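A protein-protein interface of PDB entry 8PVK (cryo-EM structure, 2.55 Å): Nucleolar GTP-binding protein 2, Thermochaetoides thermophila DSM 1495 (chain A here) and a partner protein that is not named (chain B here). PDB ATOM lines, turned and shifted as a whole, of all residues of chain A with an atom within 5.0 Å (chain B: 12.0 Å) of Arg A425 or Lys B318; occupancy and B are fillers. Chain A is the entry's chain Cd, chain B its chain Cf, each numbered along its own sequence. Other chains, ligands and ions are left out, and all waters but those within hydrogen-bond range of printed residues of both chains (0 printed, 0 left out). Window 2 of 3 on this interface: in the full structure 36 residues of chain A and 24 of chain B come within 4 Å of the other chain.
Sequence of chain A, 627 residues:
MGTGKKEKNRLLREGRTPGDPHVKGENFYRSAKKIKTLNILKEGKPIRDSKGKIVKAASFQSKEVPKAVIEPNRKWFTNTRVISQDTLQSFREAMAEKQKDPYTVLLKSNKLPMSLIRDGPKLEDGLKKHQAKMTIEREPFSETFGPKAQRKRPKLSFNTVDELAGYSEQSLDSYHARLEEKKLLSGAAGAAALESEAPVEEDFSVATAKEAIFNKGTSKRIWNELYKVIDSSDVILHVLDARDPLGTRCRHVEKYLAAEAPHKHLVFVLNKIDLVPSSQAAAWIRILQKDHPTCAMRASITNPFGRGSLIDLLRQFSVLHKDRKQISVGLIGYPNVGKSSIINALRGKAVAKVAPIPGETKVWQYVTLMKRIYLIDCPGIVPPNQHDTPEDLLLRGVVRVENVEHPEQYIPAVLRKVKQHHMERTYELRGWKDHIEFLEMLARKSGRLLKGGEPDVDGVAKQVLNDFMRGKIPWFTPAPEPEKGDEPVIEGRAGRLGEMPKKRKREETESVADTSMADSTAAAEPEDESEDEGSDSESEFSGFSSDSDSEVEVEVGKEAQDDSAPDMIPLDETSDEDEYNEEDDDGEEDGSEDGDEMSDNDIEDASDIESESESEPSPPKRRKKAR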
ATOM      1  N   HIS A 421      -5.983  30.104  -1.581  1.00  0.00           N
ATOM      2  CA  HIS A 421      -4.711  30.538  -2.152  1.00  0.00           C
ATOM      3  C   HIS A 421      -4.603  30.186  -3.630  1.00  0.00           C
ATOM      4  O   HIS A 421      -3.973  30.926  -4.395  1.00  0.00           O
ATOM      5  CB  HIS A 421      -3.543  29.941  -1.363  1.00  0.00           C
ATOM      6  CG  HIS A 421      -3.475  28.446  -1.410  1.00  0.00           C
ATOM      7  ND1 HIS A 421      -4.399  27.636  -0.788  1.00  0.00           N
ATOM      8  CD2 HIS A 421      -2.580  27.614  -1.993  1.00  0.00           C
ATOM      9  CE1 HIS A 421      -4.083  26.371  -0.993  1.00  0.00           C
ATOM     10  NE2 HIS A 421      -2.982  26.330  -1.722  1.00  0.00           N
ATOM     11  N   HIS A 422      -5.221  29.078  -4.050  1.00  0.00           N
ATOM     12  CA  HIS A 422      -5.283  28.751  -5.471  1.00  0.00           C
ATOM     13  C   HIS A 422      -6.061  29.805  -6.246  1.00  0.00           C
ATOM     14  O   HIS A 422      -5.640  30.225  -7.328  1.00  0.00           O
ATOM     15  CB  HIS A 422      -5.914  27.373  -5.668  1.00  0.00           C
ATOM     16  CG  HIS A 422      -5.072  26.245  -5.163  1.00  0.00           C
ATOM     17  ND1 HIS A 422      -3.721  26.155  -5.415  1.00  0.00           N
ATOM     18  CD2 HIS A 422      -5.389  25.158  -4.422  1.00  0.00           C
ATOM     19  CE1 HIS A 422      -3.242  25.062  -4.851  1.00  0.00           C
ATOM     20  NE2 HIS A 422      -4.233  24.439  -4.240  1.00  0.00           N
ATOM     21  N   MET A 423      -7.193  30.253  -5.697  1.00  0.00           N
ATOM     22  CA  MET A 423      -7.986  31.303  -6.332  1.00  0.00           C
ATOM     23  C   MET A 423      -7.217  32.621  -6.378  1.00  0.00           C
ATOM     24  O   MET A 423      -7.246  33.338  -7.392  1.00  0.00           O
ATOM     25  CB  MET A 423      -9.299  31.471  -5.568  1.00  0.00           C
ATOM     26  CG  MET A 423     -10.289  32.438  -6.180  1.00  0.00           C
ATOM     27  SD  MET A 423     -10.854  31.867  -7.791  1.00  0.00           S
ATOM     28  CE  MET A 423     -11.911  30.505  -7.312  1.00  0.00           C
ATOM     29  N   GLU A 424      -6.518  32.943  -5.283  1.00  0.00           N
ATOM     30  CA  GLU A 424      -5.741  34.176  -5.206  1.00  0.00           C
ATOM     31  C   GLU A 424      -4.610  34.191  -6.223  1.00  0.00           C
ATOM     32  O   GLU A 424      -4.366  35.212  -6.870  1.00  0.00           O
ATOM     33  CB  GLU A 424      -5.184  34.360  -3.795  1.00  0.00           C
ATOM     34  CG  GLU A 424      -6.223  34.706  -2.745  1.00  0.00           C
ATOM     35  CD  GLU A 424      -5.685  34.578  -1.336  1.00  0.00           C
ATOM     36  OE1 GLU A 424      -4.574  34.033  -1.170  1.00  0.00           O
ATOM     37  OE2 GLU A 424      -6.373  35.020  -0.392  1.00  0.00           O
ATOM     38  N   ARG A 425      -3.903  33.070  -6.382  1.00  0.00           N
ATOM     39  CA  ARG A 425      -2.851  33.018  -7.387  1.00  0.00           C
ATOM     40  C   ARG A 425      -3.397  32.877  -8.802  1.00  0.00           C
ATOM     41  O   ARG A 425      -2.700  33.239  -9.756  1.00  0.00           O
ATOM     42  CB  ARG A 425      -1.876  31.878  -7.088  1.00  0.00           C
ATOM     43  CG  ARG A 425      -1.076  32.085  -5.815  1.00  0.00           C
ATOM     44  CD  ARG A 425      -0.137  30.924  -5.545  1.00  0.00           C
ATOM     45  NE  ARG A 425      -0.846  29.693  -5.226  1.00  0.00           N
ATOM     46  CZ  ARG A 425      -0.260  28.512  -5.085  1.00  0.00           C
ATOM     47  NH1 ARG A 425       1.048  28.369  -5.219  1.00  0.00           N
ATOM     48  NH2 ARG A 425      -1.006  27.448  -4.804  1.00  0.00           N
ATOM     49  N   THR A 426      -4.617  32.359  -8.958  1.00  0.00           N
ATOM     50  CA  THR A 426      -5.223  32.284 -10.282  1.00  0.00           C
ATOM     51  C   THR A 426      -5.591  33.667 -10.800  1.00  0.00           C
ATOM     52  O   THR A 426      -5.323  33.992 -11.963  1.00  0.00           O
ATOM     53  CB  THR A 426      -6.460  31.384 -10.242  1.00  0.00           C
ATOM     54  OG1 THR A 426      -6.089  30.079  -9.783  1.00  0.00           O
ATOM     55  CG2 THR A 426      -7.088  31.265 -11.622  1.00  0.00           C
ATOM     56  N   TYR A 427      -6.194  34.504  -9.955  1.00  0.00           N
ATOM     57  CA  TYR A 427      -6.674  35.802 -10.416  1.00  0.00           C
ATOM     58  C   TYR A 427      -5.834  36.980  -9.937  1.00  0.00           C
ATOM     59  O   TYR A 427      -6.209  38.126 -10.205  1.00  0.00           O
ATOM     60  CB  TYR A 427      -8.137  35.996 -10.016  1.00  0.00           C
ATOM     61  CG  TYR A 427      -9.082  35.158 -10.843  1.00  0.00           C
ATOM     62  CD1 TYR A 427      -9.280  35.431 -12.190  1.00  0.00           C
ATOM     63  CD2 TYR A 427      -9.764  34.088 -10.284  1.00  0.00           C
ATOM     64  CE1 TYR A 427     -10.138  34.665 -12.955  1.00  0.00           C
ATOM     65  CE2 TYR A 427     -10.624  33.316 -11.041  1.00  0.00           C
ATOM     66  CZ  TYR A 427     -10.806  33.610 -12.375  1.00  0.00           C
ATOM     67  OH  TYR A 427     -11.663  32.843 -13.129  1.00  0.00           O
ATOM     68  N   GLU A 428      -4.699  36.725  -9.271  1.00  0.00           N
ATOM     69  CA  GLU A 428      -3.795  37.762  -8.751  1.00  0.00           C
ATOM     70  C   GLU A 428      -4.534  38.770  -7.874  1.00  0.00           C
ATOM     71  O   GLU A 428      -4.309  39.980  -7.949  1.00  0.00           O
ATOM     72  CB  GLU A 428      -3.044  38.465  -9.885  1.00  0.00           C
ATOM     73  CG  GLU A 428      -2.244  37.525 -10.772  1.00  0.00           C
ATOM     74  CD  GLU A 428      -2.060  38.061 -12.178  1.00  0.00           C
ATOM     75  OE1 GLU A 428      -1.141  38.880 -12.388  1.00  0.00           O
ATOM     76  OE2 GLU A 428      -2.833  37.663 -13.074  1.00  0.00           O
ATOM     77  N   ARG A 430      -6.161  39.451  -3.847  1.00  0.00           N
ATOM     78  CA  ARG A 430      -6.147  39.078  -2.440  1.00  0.00           C
ATOM     79  C   ARG A 430      -7.105  39.961  -1.654  1.00  0.00           C
ATOM     80  O   ARG A 430      -7.345  41.116  -2.010  1.00  0.00           O
ATOM     81  CB  ARG A 430      -4.742  39.199  -1.808  1.00  0.00           C
ATOM     82  CG  ARG A 430      -3.801  38.001  -1.978  1.00  0.00           C
ATOM     83  CD  ARG A 430      -3.318  37.810  -3.407  1.00  0.00           C
ATOM     84  NE  ARG A 430      -2.312  36.759  -3.507  1.00  0.00           N
ATOM     85  CZ  ARG A 430      -1.801  36.316  -4.648  1.00  0.00           C
ATOM     86  NH1 ARG A 430      -2.175  36.819  -5.813  1.00  0.00           N
ATOM     87  NH2 ARG A 430      -0.893  35.346  -4.619  1.00  0.00           N
ATOM     88  N   GLN B 310       2.754  13.933 -16.620  1.00  0.00           N
ATOM     89  CA  GLN B 310       2.981  15.324 -16.258  1.00  0.00           C
ATOM     90  C   GLN B 310       1.634  16.016 -16.104  1.00  0.00           C
ATOM     91  O   GLN B 310       0.858  16.091 -17.062  1.00  0.00           O
ATOM     92  CB  GLN B 310       3.835  16.030 -17.310  1.00  0.00           C
ATOM     93  CG  GLN B 310       5.325  15.804 -17.142  1.00  0.00           C
ATOM     94  CD  GLN B 310       5.860  16.427 -15.872  1.00  0.00           C
ATOM     95  OE1 GLN B 310       5.610  17.598 -15.591  1.00  0.00           O
ATOM     96  NE2 GLN B 310       6.594  15.644 -15.092  1.00  0.00           N
ATOM     97  N   THR B 311       1.358  16.513 -14.902  1.00  0.00           N
ATOM     98  CA  THR B 311       0.113  17.223 -14.660  1.00  0.00           C
ATOM     99  C   THR B 311       0.154  18.602 -15.312  1.00  0.00           C
ATOM    100  O   THR B 311       1.213  19.113 -15.687  1.00  0.00           O
ATOM    101  CB  THR B 311      -0.154  17.352 -13.160  1.00  0.00           C
ATOM    102  OG1 THR B 311       1.058  17.712 -12.485  1.00  0.00           O
ATOM    103  CG2 THR B 311      -0.662  16.037 -12.601  1.00  0.00           C
ATOM    104  N   ARG B 312      -1.026  19.199 -15.457  1.00  0.00           N
ATOM    105  CA  ARG B 312      -1.140  20.491 -16.118  1.00  0.00           C
ATOM    106  C   ARG B 312      -0.551  21.591 -15.244  1.00  0.00           C
ATOM    107  O   ARG B 312      -0.869  21.692 -14.055  1.00  0.00           O
ATOM    108  CB  ARG B 312      -2.604  20.790 -16.436  1.00  0.00           C
ATOM    109  CG  ARG B 312      -2.825  22.048 -17.255  1.00  0.00           C
ATOM    110  CD  ARG B 312      -4.215  22.055 -17.868  1.00  0.00           C
ATOM    111  NE  ARG B 312      -4.397  23.148 -18.815  1.00  0.00           N
ATOM    112  CZ  ARG B 312      -4.011  23.114 -20.083  1.00  0.00           C
ATOM    113  NH1 ARG B 312      -3.416  22.051 -20.597  1.00  0.00           N
ATOM    114  NH2 ARG B 312      -4.233  24.172 -20.857  1.00  0.00           N
ATOM    115  N   LYS B 313       0.309  22.420 -15.838  1.00  0.00           N
ATOM    116  CA  LYS B 313       0.955  23.519 -15.121  1.00  0.00           C
ATOM    117  C   LYS B 313       0.011  24.717 -15.130  1.00  0.00           C
ATOM    118  O   LYS B 313       0.132  25.649 -15.929  1.00  0.00           O
ATOM    119  CB  LYS B 313       2.304  23.860 -15.745  1.00  0.00           C
ATOM    120  CG  LYS B 313       3.210  22.666 -15.997  1.00  0.00           C
ATOM    121  CD  LYS B 313       3.422  21.840 -14.738  1.00  0.00           C
ATOM    122  CE  LYS B 313       4.153  20.549 -15.053  1.00  0.00           C
ATOM    123  NZ  LYS B 313       3.905  19.504 -14.025  1.00  0.00           N
ATOM    124  N   MET B 314      -0.952  24.683 -14.216  1.00  0.00           N
ATOM    125  CA  MET B 314      -1.958  25.727 -14.135  1.00  0.00           C
ATOM    126  C   MET B 314      -1.385  26.984 -13.488  1.00  0.00           C
ATOM    127  O   MET B 314      -0.364  26.951 -12.796  1.00  0.00           O
ATOM    128  CB  MET B 314      -3.176  25.237 -13.354  1.00  0.00           C
ATOM    129  CG  MET B 314      -3.977  24.172 -14.081  1.00  0.00           C
ATOM    130  SD  MET B 314      -5.662  24.008 -13.467  1.00  0.00           S
ATOM    131  CE  MET B 314      -5.608  22.348 -12.798  1.00  0.00           C
ATOM    132  N   LYS B 315      -2.061  28.108 -13.741  1.00  0.00           N
ATOM    133  CA  LYS B 315      -1.629  29.389 -13.190  1.00  0.00           C
ATOM    134  C   LYS B 315      -1.763  29.417 -11.672  1.00  0.00           C
ATOM    135  O   LYS B 315      -0.923  30.002 -10.980  1.00  0.00           O
ATOM    136  CB  LYS B 315      -2.435  30.521 -13.825  1.00  0.00           C
ATOM    137  CG  LYS B 315      -1.936  31.917 -13.499  1.00  0.00           C
ATOM    138  CD  LYS B 315      -2.888  32.970 -14.040  1.00  0.00           C
ATOM    139  CE  LYS B 315      -2.287  34.361 -13.945  1.00  0.00           C
ATOM    140  NZ  LYS B 315      -3.262  35.413 -14.345  1.00  0.00           N
ATOM    141  N   GLY B 316      -2.812  28.788 -11.137  1.00  0.00           N
ATOM    142  CA  GLY B 316      -3.019  28.768  -9.701  1.00  0.00           C
ATOM    143  C   GLY B 316      -2.069  27.862  -8.949  1.00  0.00           C
ATOM    144  O   GLY B 316      -1.949  27.989  -7.727  1.00  0.00           O
ATOM    145  N   LEU B 317      -1.395  26.952  -9.646  1.00  0.00           N
ATOM    146  CA  LEU B 317      -0.440  26.047  -9.025  1.00  0.00           C
ATOM    147  C   LEU B 317       0.987  26.573  -9.061  1.00  0.00           C
ATOM    148  O   LEU B 317       1.900  25.874  -8.607  1.00  0.00           O
ATOM    149  CB  LEU B 317      -0.496  24.674  -9.703  1.00  0.00           C
ATOM    150  CG  LEU B 317      -1.719  23.822  -9.373  1.00  0.00           C
ATOM    151  CD1 LEU B 317      -1.614  22.460 -10.035  1.00  0.00           C
ATOM    152  CD2 LEU B 317      -1.877  23.684  -7.872  1.00  0.00           C
ATOM    153  N   LYS B 318       1.204  27.775  -9.583  1.00  0.00           N
ATOM    154  CA  LYS B 318       2.528  28.373  -9.649  1.00  0.00           C
ATOM    155  C   LYS B 318       2.712  29.352  -8.498  1.00  0.00           C
ATOM    156  O   LYS B 318       1.780  30.065  -8.119  1.00  0.00           O
ATOM    157  CB  LYS B 318       2.743  29.086 -10.985  1.00  0.00           C
ATOM    158  CG  LYS B 318       2.741  28.156 -12.185  1.00  0.00           C
ATOM    159  CD  LYS B 318       2.910  28.923 -13.485  1.00  0.00           C
ATOM    160  CE  LYS B 318       3.011  27.975 -14.669  1.00  0.00           C
ATOM    161  NZ  LYS B 318       3.100  28.703 -15.963  1.00  0.00           N
ATOM    162  N   ARG B 319       3.920  29.377  -7.946  1.00  0.00           N
ATOM    163  CA  ARG B 319       4.224  30.220  -6.794  1.00  0.00           C
ATOM    164  C   ARG B 319       4.375  31.680  -7.210  1.00  0.00           C
ATOM    165  O   ARG B 319       5.470  32.130  -7.544  1.00  0.00           O
ATOM    166  CB  ARG B 319       5.499  29.739  -6.092  1.00  0.00           C
ATOM    167  CG  ARG B 319       5.320  28.526  -5.176  1.00  0.00           C
ATOM    168  CD  ARG B 319       5.327  27.210  -5.944  1.00  0.00           C
ATOM    169  NE  ARG B 319       6.617  26.948  -6.569  1.00  0.00           N
ATOM    170  CZ  ARG B 319       6.829  26.016  -7.490  1.00  0.00           C
ATOM    171  NH1 ARG B 319       5.851  25.239  -7.925  1.00  0.00           N
ATOM    172  NH2 ARG B 319       8.053  25.864  -7.989  1.00  0.00           N
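Of the 10 printed residues of chain B, 5 touch a printed residue of chain A. Hydrophobic or aromatic side chains of chain B that line the printed part of chain A: Leu B317. Of the 9 printed residues of chain A, 4 touch a printed residue of chain B.
CD2 of Leu B317 touches CE1 of His A422, 3.6 Å away. O of Arg A425 touches O of Lys B315 (3.9 Å). NH1 of Arg A425 touches CA of Arg B319, at 3.999 Å. Thr A426 touches Gly B316.
A ring nitrogen (ND1) of His A422 is in hydrogen-bond range of the guanidinium group (NH2) of Arg A425 (3.1 Å). O of His A422 is in hydrogen-bond range of OG1 of Thr A426, at 2.5 Å. A ring nitrogen (NE2) of His A421 lies close to a ring nitrogen (NE2) of His A422 (3.4 Å). O of His A421 sits close to NE of Arg A425, 3.5 Å away.
The backbone carbonyl oxygen (O) of Lys B318 sits close to the guanidinium group (NH1) of Arg A425. O of Thr A426 sits close to NZ of Lys B315 (3.5 Å). OE2 of Glu A428 is in salt-bridge range of NZ of Lys B315, at 2.6 Å. A ring nitrogen (ND1) of His A422 sits at hydrogen-bond distance from the backbone carbonyl oxygen (O) of Gly B316 (3.4 Å). NH2 of Arg A425 lies within hydrogen-bond range of O of Gly B316.
Of chain B, only Gly B316 and Leu B317 come within 4 Å of His A422. No residue of chain B comes within 4 Å of Glu A424. Printed residues of chain B within 4 Å of Arg A425: Lys B315, Gly B316, Lys B318 and Arg B319. Of chain B, only Lys B315 comes within 4 Å of Glu A428. Gln B310 touches none of the printed residues of chain A. Of the printed residues of chain A, Lys B315 touches Arg A425, Thr A426 and Glu A428. Printed residues of chain A within 4 Å of Leu B317: His A422. The nearest printed residue of chain B that does not touch Arg A425 is Leu B317 (4.2 Å). The nearest printed residue of chain A that does not touch Gly B316 is His A421 (4.9 Å).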
